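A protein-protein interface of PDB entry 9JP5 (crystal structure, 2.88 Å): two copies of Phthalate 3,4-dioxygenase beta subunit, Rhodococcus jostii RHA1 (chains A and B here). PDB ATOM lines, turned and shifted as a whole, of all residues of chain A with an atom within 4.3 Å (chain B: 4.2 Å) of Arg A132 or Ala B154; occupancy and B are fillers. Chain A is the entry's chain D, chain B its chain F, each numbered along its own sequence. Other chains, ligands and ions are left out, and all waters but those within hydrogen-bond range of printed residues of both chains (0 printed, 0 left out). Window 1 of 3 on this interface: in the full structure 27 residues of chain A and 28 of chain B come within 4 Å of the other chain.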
ATOM      1  N   TYR A  60       8.996 -16.184  26.186  1.00  0.00           N
ATOM      2  CA  TYR A  60       9.206 -16.193  24.747  1.00  0.00           C
ATOM      3  C   TYR A  60      10.694 -15.992  24.502  1.00  0.00           C
ATOM      4  O   TYR A  60      11.250 -16.644  23.616  1.00  0.00           O
ATOM      5  CB  TYR A  60       8.285 -15.253  23.963  1.00  0.00           C
ATOM      6  CG  TYR A  60       6.927 -15.917  23.801  1.00  0.00           C
ATOM      7  CD1 TYR A  60       5.987 -15.870  24.819  1.00  0.00           C
ATOM      8  CD2 TYR A  60       6.622 -16.670  22.686  1.00  0.00           C
ATOM      9  CE1 TYR A  60       4.766 -16.517  24.732  1.00  0.00           C
ATOM     10  CE2 TYR A  60       5.403 -17.321  22.579  1.00  0.00           C
ATOM     11  CZ  TYR A  60       4.468 -17.245  23.600  1.00  0.00           C
ATOM     12  OH  TYR A  60       3.250 -17.872  23.498  1.00  0.00           O
ATOM     13  N   ASP A  63      12.618 -19.297  25.457  1.00  0.00           N
ATOM     14  CA  ASP A  63      12.355 -20.334  24.467  1.00  0.00           C
ATOM     15  C   ASP A  63      13.304 -20.150  23.283  1.00  0.00           C
ATOM     16  O   ASP A  63      13.966 -21.098  22.865  1.00  0.00           O
ATOM     17  CB  ASP A  63      10.911 -20.313  23.954  1.00  0.00           C
ATOM     18  CG  ASP A  63       9.865 -20.897  24.885  1.00  0.00           C
ATOM     19  OD1 ASP A  63      10.250 -21.419  25.933  1.00  0.00           O
ATOM     20  OD2 ASP A  63       8.663 -20.830  24.543  1.00  0.00           O
ATOM     21  N   LEU A 131      13.071 -25.750  23.524  1.00  0.00           N
ATOM     22  CA  LEU A 131      12.666 -25.392  24.879  1.00  0.00           C
ATOM     23  C   LEU A 131      11.246 -24.840  24.912  1.00  0.00           C
ATOM     24  O   LEU A 131      10.791 -24.180  23.977  1.00  0.00           O
ATOM     25  CB  LEU A 131      13.664 -24.381  25.458  1.00  0.00           C
ATOM     26  CG  LEU A 131      15.110 -24.872  25.550  1.00  0.00           C
ATOM     27  CD1 LEU A 131      16.020 -23.741  25.998  1.00  0.00           C
ATOM     28  CD2 LEU A 131      15.235 -26.069  26.487  1.00  0.00           C
ATOM     29  N   ARG A 132      10.571 -25.108  26.033  1.00  0.00           N
ATOM     30  CA  ARG A 132       9.214 -24.639  26.243  1.00  0.00           C
ATOM     31  C   ARG A 132       9.066 -24.335  27.724  1.00  0.00           C
ATOM     32  O   ARG A 132       8.788 -25.222  28.518  1.00  0.00           O
ATOM     33  CB  ARG A 132       8.187 -25.666  25.755  1.00  0.00           C
ATOM     34  CG  ARG A 132       6.803 -25.100  25.486  1.00  0.00           C
ATOM     35  CD  ARG A 132       6.747 -24.040  24.388  1.00  0.00           C
ATOM     36  NE  ARG A 132       6.962 -24.525  23.025  1.00  0.00           N
ATOM     37  CZ  ARG A 132       7.403 -23.771  22.016  1.00  0.00           C
ATOM     38  NH1 ARG A 132       7.674 -22.486  22.202  1.00  0.00           N
ATOM     39  NH2 ARG A 132       7.610 -24.313  20.825  1.00  0.00           N
ATOM     40  N   HIS A 133       9.288 -23.071  28.079  1.00  0.00           N
ATOM     41  CA  HIS A 133       8.969 -22.620  29.417  1.00  0.00           C
ATOM     42  C   HIS A 133       7.463 -22.316  29.499  1.00  0.00           C
ATOM     43  O   HIS A 133       6.997 -21.285  28.989  1.00  0.00           O
ATOM     44  CB  HIS A 133       9.830 -21.411  29.792  1.00  0.00           C
ATOM     45  CG  HIS A 133      11.297 -21.575  29.608  1.00  0.00           C
ATOM     46  ND1 HIS A 133      11.866 -21.755  28.369  1.00  0.00           N
ATOM     47  CD2 HIS A 133      12.313 -21.517  30.477  1.00  0.00           C
ATOM     48  CE1 HIS A 133      13.181 -21.838  28.496  1.00  0.00           C
ATOM     49  NE2 HIS A 133      13.474 -21.698  29.770  1.00  0.00           N
ATOM     50  N   TYR A 134       6.718 -23.241  30.123  1.00  0.00           N
ATOM     51  CA  TYR A 134       5.326 -23.024  30.462  1.00  0.00           C
ATOM     52  C   TYR A 134       5.253 -22.255  31.775  1.00  0.00           C
ATOM     53  O   TYR A 134       5.875 -22.653  32.750  1.00  0.00           O
ATOM     54  CB  TYR A 134       4.620 -24.365  30.623  1.00  0.00           C
ATOM     55  CG  TYR A 134       4.483 -25.170  29.345  1.00  0.00           C
ATOM     56  CD1 TYR A 134       3.402 -24.984  28.497  1.00  0.00           C
ATOM     57  CD2 TYR A 134       5.433 -26.115  28.982  1.00  0.00           C
ATOM     58  CE1 TYR A 134       3.253 -25.714  27.333  1.00  0.00           C
ATOM     59  CE2 TYR A 134       5.311 -26.838  27.802  1.00  0.00           C
ATOM     60  CZ  TYR A 134       4.216 -26.639  26.977  1.00  0.00           C
ATOM     61  OH  TYR A 134       4.064 -27.353  25.823  1.00  0.00           O
ATOM     62  N   LEU A 156       7.038 -24.851  34.393  1.00  0.00           N
ATOM     63  CA  LEU A 156       7.332 -26.203  33.955  1.00  0.00           C
ATOM     64  C   LEU A 156       8.116 -26.126  32.663  1.00  0.00           C
ATOM     65  O   LEU A 156       7.545 -25.796  31.640  1.00  0.00           O
ATOM     66  CB  LEU A 156       6.027 -26.973  33.719  1.00  0.00           C
ATOM     67  CG  LEU A 156       6.185 -28.378  33.127  1.00  0.00           C
ATOM     68  CD1 LEU A 156       6.665 -29.376  34.173  1.00  0.00           C
ATOM     69  CD2 LEU A 156       4.882 -28.851  32.485  1.00  0.00           C
ATOM     70  N   LEU A 157       9.401 -26.476  32.710  1.00  0.00           N
ATOM     71  CA  LEU A 157      10.237 -26.495  31.519  1.00  0.00           C
ATOM     72  C   LEU A 157      10.197 -27.883  30.886  1.00  0.00           C
ATOM     73  O   LEU A 157      10.551 -28.855  31.538  1.00  0.00           O
ATOM     74  CB  LEU A 157      11.673 -26.105  31.891  1.00  0.00           C
ATOM     75  CG  LEU A 157      12.704 -26.388  30.802  1.00  0.00           C
ATOM     76  CD1 LEU A 157      12.388 -25.630  29.518  1.00  0.00           C
ATOM     77  CD2 LEU A 157      14.096 -26.039  31.286  1.00  0.00           C
ATOM     78  N   PHE A 158       9.778 -27.945  29.615  1.00  0.00           N
ATOM     79  CA  PHE A 158       9.933 -29.125  28.774  1.00  0.00           C
ATOM     80  C   PHE A 158      11.151 -28.929  27.866  1.00  0.00           C
ATOM     81  O   PHE A 158      11.344 -27.834  27.324  1.00  0.00           O
ATOM     82  CB  PHE A 158       8.652 -29.346  27.971  1.00  0.00           C
ATOM     83  CG  PHE A 158       8.682 -30.470  26.972  1.00  0.00           C
ATOM     84  CD1 PHE A 158       9.493 -30.409  25.846  1.00  0.00           C
ATOM     85  CD2 PHE A 158       7.849 -31.563  27.124  1.00  0.00           C
ATOM     86  CE1 PHE A 158       9.503 -31.439  24.918  1.00  0.00           C
ATOM     87  CE2 PHE A 158       7.852 -32.587  26.186  1.00  0.00           C
ATOM     88  CZ  PHE A 158       8.676 -32.522  25.088  1.00  0.00           C
ATOM     89  N   TYR B 134      -3.499 -28.516  27.585  1.00  0.00           N
ATOM     90  CA  TYR B 134      -3.170 -27.422  28.480  1.00  0.00           C
ATOM     91  C   TYR B 134      -2.698 -26.232  27.653  1.00  0.00           C
ATOM     92  O   TYR B 134      -1.721 -26.377  26.929  1.00  0.00           O
ATOM     93  CB  TYR B 134      -2.074 -27.825  29.469  1.00  0.00           C
ATOM     94  CG  TYR B 134      -2.499 -28.843  30.526  1.00  0.00           C
ATOM     95  CD1 TYR B 134      -2.461 -30.209  30.270  1.00  0.00           C
ATOM     96  CD2 TYR B 134      -2.946 -28.442  31.787  1.00  0.00           C
ATOM     97  CE1 TYR B 134      -2.835 -31.133  31.230  1.00  0.00           C
ATOM     98  CE2 TYR B 134      -3.339 -29.362  32.748  1.00  0.00           C
ATOM     99  CZ  TYR B 134      -3.264 -30.715  32.476  1.00  0.00           C
ATOM    100  OH  TYR B 134      -3.611 -31.633  33.426  1.00  0.00           O
ATOM    101  N   ILE B 135      -3.349 -25.059  27.772  1.00  0.00           N
ATOM    102  CA  ILE B 135      -2.938 -23.879  27.021  1.00  0.00           C
ATOM    103  C   ILE B 135      -2.355 -22.823  27.953  1.00  0.00           C
ATOM    104  O   ILE B 135      -2.976 -22.456  28.935  1.00  0.00           O
ATOM    105  CB  ILE B 135      -4.131 -23.302  26.251  1.00  0.00           C
ATOM    106  CG1 ILE B 135      -5.004 -24.409  25.647  1.00  0.00           C
ATOM    107  CG2 ILE B 135      -3.645 -22.296  25.215  1.00  0.00           C
ATOM    108  CD1 ILE B 135      -4.287 -25.322  24.684  1.00  0.00           C
ATOM    109  N   THR B 136      -1.181 -22.294  27.628  1.00  0.00           N
ATOM    110  CA  THR B 136      -0.596 -21.281  28.489  1.00  0.00           C
ATOM    111  C   THR B 136       0.154 -20.260  27.633  1.00  0.00           C
ATOM    112  O   THR B 136       0.172 -20.341  26.413  1.00  0.00           O
ATOM    113  CB  THR B 136       0.220 -21.955  29.605  1.00  0.00           C
ATOM    114  OG1 THR B 136       0.069 -21.181  30.790  1.00  0.00           O
ATOM    115  CG2 THR B 136       1.701 -22.081  29.338  1.00  0.00           C
ATOM    116  N   ASN B 137       0.747 -19.266  28.295  1.00  0.00           N
ATOM    117  CA  ASN B 137       1.716 -18.368  27.683  1.00  0.00           C
ATOM    118  C   ASN B 137       1.088 -17.619  26.513  1.00  0.00           C
ATOM    119  O   ASN B 137       1.771 -17.348  25.535  1.00  0.00           O
ATOM    120  CB  ASN B 137       2.992 -19.101  27.243  1.00  0.00           C
ATOM    121  CG  ASN B 137       3.901 -19.518  28.392  1.00  0.00           C
ATOM    122  OD1 ASN B 137       3.488 -19.590  29.554  1.00  0.00           O
ATOM    123  ND2 ASN B 137       5.147 -19.841  28.072  1.00  0.00           N
ATOM    124  N   SER B 153       0.753 -19.045  21.667  1.00  0.00           N
ATOM    125  CA  SER B 153       0.418 -19.834  22.834  1.00  0.00           C
ATOM    126  C   SER B 153       1.423 -20.970  22.942  1.00  0.00           C
ATOM    127  O   SER B 153       2.110 -21.292  21.985  1.00  0.00           O
ATOM    128  CB  SER B 153      -1.013 -20.349  22.783  1.00  0.00           C
ATOM    129  OG  SER B 153      -1.301 -21.010  21.553  1.00  0.00           O
ATOM    130  N   ALA B 154       1.529 -21.530  24.147  1.00  0.00           N
ATOM    131  CA  ALA B 154       2.143 -22.824  24.358  1.00  0.00           C
ATOM    132  C   ALA B 154       1.033 -23.808  24.701  1.00  0.00           C
ATOM    133  O   ALA B 154       0.154 -23.500  25.502  1.00  0.00           O
ATOM    134  CB  ALA B 154       3.175 -22.743  25.460  1.00  0.00           C
ATOM    135  N   GLU B 155       1.092 -24.993  24.098  1.00  0.00           N
ATOM    136  CA  GLU B 155       0.092 -26.025  24.301  1.00  0.00           C
ATOM    137  C   GLU B 155       0.810 -27.321  24.650  1.00  0.00           C
ATOM    138  O   GLU B 155       1.654 -27.772  23.872  1.00  0.00           O
ATOM    139  CB  GLU B 155      -0.755 -26.196  23.037  1.00  0.00           C
ATOM    140  CG  GLU B 155      -1.589 -27.451  23.050  1.00  0.00           C
ATOM    141  CD  GLU B 155      -2.648 -27.498  21.969  1.00  0.00           C
ATOM    142  OE1 GLU B 155      -3.829 -27.719  22.301  1.00  0.00           O
ATOM    143  OE2 GLU B 155      -2.284 -27.316  20.794  1.00  0.00           O
ATOM    144  N   SER B 171       4.485 -31.463  23.618  1.00  0.00           N
ATOM    145  CA  SER B 171       4.773 -30.065  23.862  1.00  0.00           C
ATOM    146  C   SER B 171       4.912 -29.360  22.516  1.00  0.00           C
ATOM    147  O   SER B 171       5.485 -29.912  21.588  1.00  0.00           O
ATOM    148  CB  SER B 171       6.018 -29.939  24.679  1.00  0.00           C
ATOM    149  OG  SER B 171       6.279 -28.584  24.972  1.00  0.00           O
ATOM    150  N   CYS B 172       4.358 -28.154  22.403  1.00  0.00           N
ATOM    151  CA  CYS B 172       4.477 -27.358  21.193  1.00  0.00           C
ATOM    152  C   CYS B 172       4.274 -25.882  21.524  1.00  0.00           C
ATOM    153  O   CYS B 172       3.834 -25.533  22.615  1.00  0.00           O
ATOM    154  CB  CYS B 172       3.463 -27.764  20.130  1.00  0.00           C
ATOM    155  SG  CYS B 172       1.754 -27.454  20.639  1.00  0.00           S
ATOM    156  N   GLY B 173       4.662 -25.043  20.561  1.00  0.00           N
ATOM    157  CA  GLY B 173       4.237 -23.662  20.453  1.00  0.00           C
ATOM    158  C   GLY B 173       3.364 -23.477  19.215  1.00  0.00           C
ATOM    159  O   GLY B 173       3.442 -24.247  18.258  1.00  0.00           O
ATOM    160  N   PHE B 193       4.697 -25.518  16.325  1.00  0.00           N
ATOM    161  CA  PHE B 193       6.102 -25.820  16.459  1.00  0.00           C
ATOM    162  C   PHE B 193       6.241 -26.947  17.471  1.00  0.00           C
ATOM    163  O   PHE B 193       6.242 -26.708  18.676  1.00  0.00           O
ATOM    164  CB  PHE B 193       6.860 -24.579  16.909  1.00  0.00           C
ATOM    165  CG  PHE B 193       6.608 -23.358  16.061  1.00  0.00           C
ATOM    166  CD1 PHE B 193       5.498 -22.541  16.286  1.00  0.00           C
ATOM    167  CD2 PHE B 193       7.501 -22.996  15.059  1.00  0.00           C
ATOM    168  CE1 PHE B 193       5.267 -21.409  15.513  1.00  0.00           C
ATOM    169  CE2 PHE B 193       7.269 -21.862  14.286  1.00  0.00           C
ATOM    170  CZ  PHE B 193       6.154 -21.071  14.517  1.00  0.00           C
ATOM    171  N   ASP B 195       7.872 -29.730  19.767  1.00  0.00           N
ATOM    172  CA  ASP B 195       9.114 -29.622  20.515  1.00  0.00           C
ATOM    173  C   ASP B 195       9.920 -30.918  20.461  1.00  0.00           C
ATOM    174  O   ASP B 195      10.978 -31.005  21.068  1.00  0.00           O
ATOM    175  CB  ASP B 195       8.827 -29.222  21.960  1.00  0.00           C
ATOM    176  CG  ASP B 195       8.221 -27.837  22.067  1.00  0.00           C
ATOM    177  OD1 ASP B 195       8.685 -26.962  21.331  1.00  0.00           O
ATOM    178  OD2 ASP B 195       7.287 -27.653  22.874  1.00  0.00           O
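The side-chain carboxylate (OD2) of Asp A63 lies within salt-bridge range of the guanidinium group (NH1) of Arg A132, at 3.0 Å.
The backbone carbonyl oxygen of Arg A132 is in hydrogen-bond range of the backbone NH of Phe A158.
O of Ala B154 lies within hydrogen-bond range of N of Thr B136, 2.8 Å away.
O of Glu B155 is in hydrogen-bond range of N of Cys B172, at 3.1 Å.
The side-chain carboxylate (OD2) of Asp B195 is in hydrogen-bond range of the backbone NH (N) of Cys B172.
The backbone NH (N) of Phe B193 lies within hydrogen-bond range of the backbone carbonyl oxygen (O) of Gly B173 (2.6 Å).
Of chain B, only Ala B154 (3.9 Å), Ser B171 (3.6 Å), Cys B172 (3.3 Å), Gly B173 (3.0 Å), Phe B193 (3.5 Å) and Asp B195 (2.9 Å) come within 4 Å of Arg A132.
Of the printed residues of chain A, Ser B171 touches Arg A132, Tyr A134 and Phe A158.
Printed residues of chain A within 4 Å of Asp B195: Arg A132 and Phe A158.
Printed residues of chain A within 4 Å of Asn B137: Tyr A60 (2.6 Å), His A133 (2.5 Å) and Tyr A134 (3.9 Å).
Printed residues of chain A within 4 Å of Phe B193: Arg A132.
Ile B135 touches none of the printed residues of chain A.
Leu A131 touches none of the printed residues of chain B.
The nearest printed residue of chain B that does not touch Arg A132 is Ser B153 (5.7 Å).
The nearest printed residue of chain A that does not touch Asn B137 is Asp A63 (5.1 Å).
1 position is printed for both chains.
OH of Tyr A60 lies within hydrogen-bond range of O of Asn B137 (2.6 Å).
The side-chain hydroxyl (OH) of Tyr A60 sits at hydrogen-bond distance from the backbone NH (N) of Ser B153.
The backbone carbonyl oxygen (O) of Cys B172 lies within hydrogen-bond range of the guanidinium group (NE) of Arg A132 (3.3 Å).
O of Phe B193 lies within hydrogen-bond range of NH2 of Arg A132 (3.5 Å).
OD1 of Asp B195 lies within salt-bridge range of NH2 of Arg A132 (2.9 Å).
The backbone carbonyl oxygen (O) of His A133 sits at hydrogen-bond distance from the side-chain amide nitrogen (ND2) of Asn B137 (2.5 Å).
The backbone carbonyl oxygen (O) of Glu B155 is in hydrogen-bond range of the side-chain hydroxyl (OH) of Tyr A134 (3.1 Å).
OG of Ser B171 sits at hydrogen-bond distance from OH of Tyr A134 (2.7 Å).
The backbone NH (N) of Gly B173 lies close to the guanidinium group (NH2) of Arg A132, 3.0 Å away.
Among the printed residues, merely in contact across the chains: Arg A132 with Ala B154, Arg A132 with Ser B171, Tyr A134 with Thr B136, Tyr A134 with Asn B137, Tyr A134 with Ala B154, Tyr A134 with Cys B172, Phe A158 with Ser B171 and Phe A158 with Asp B195.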
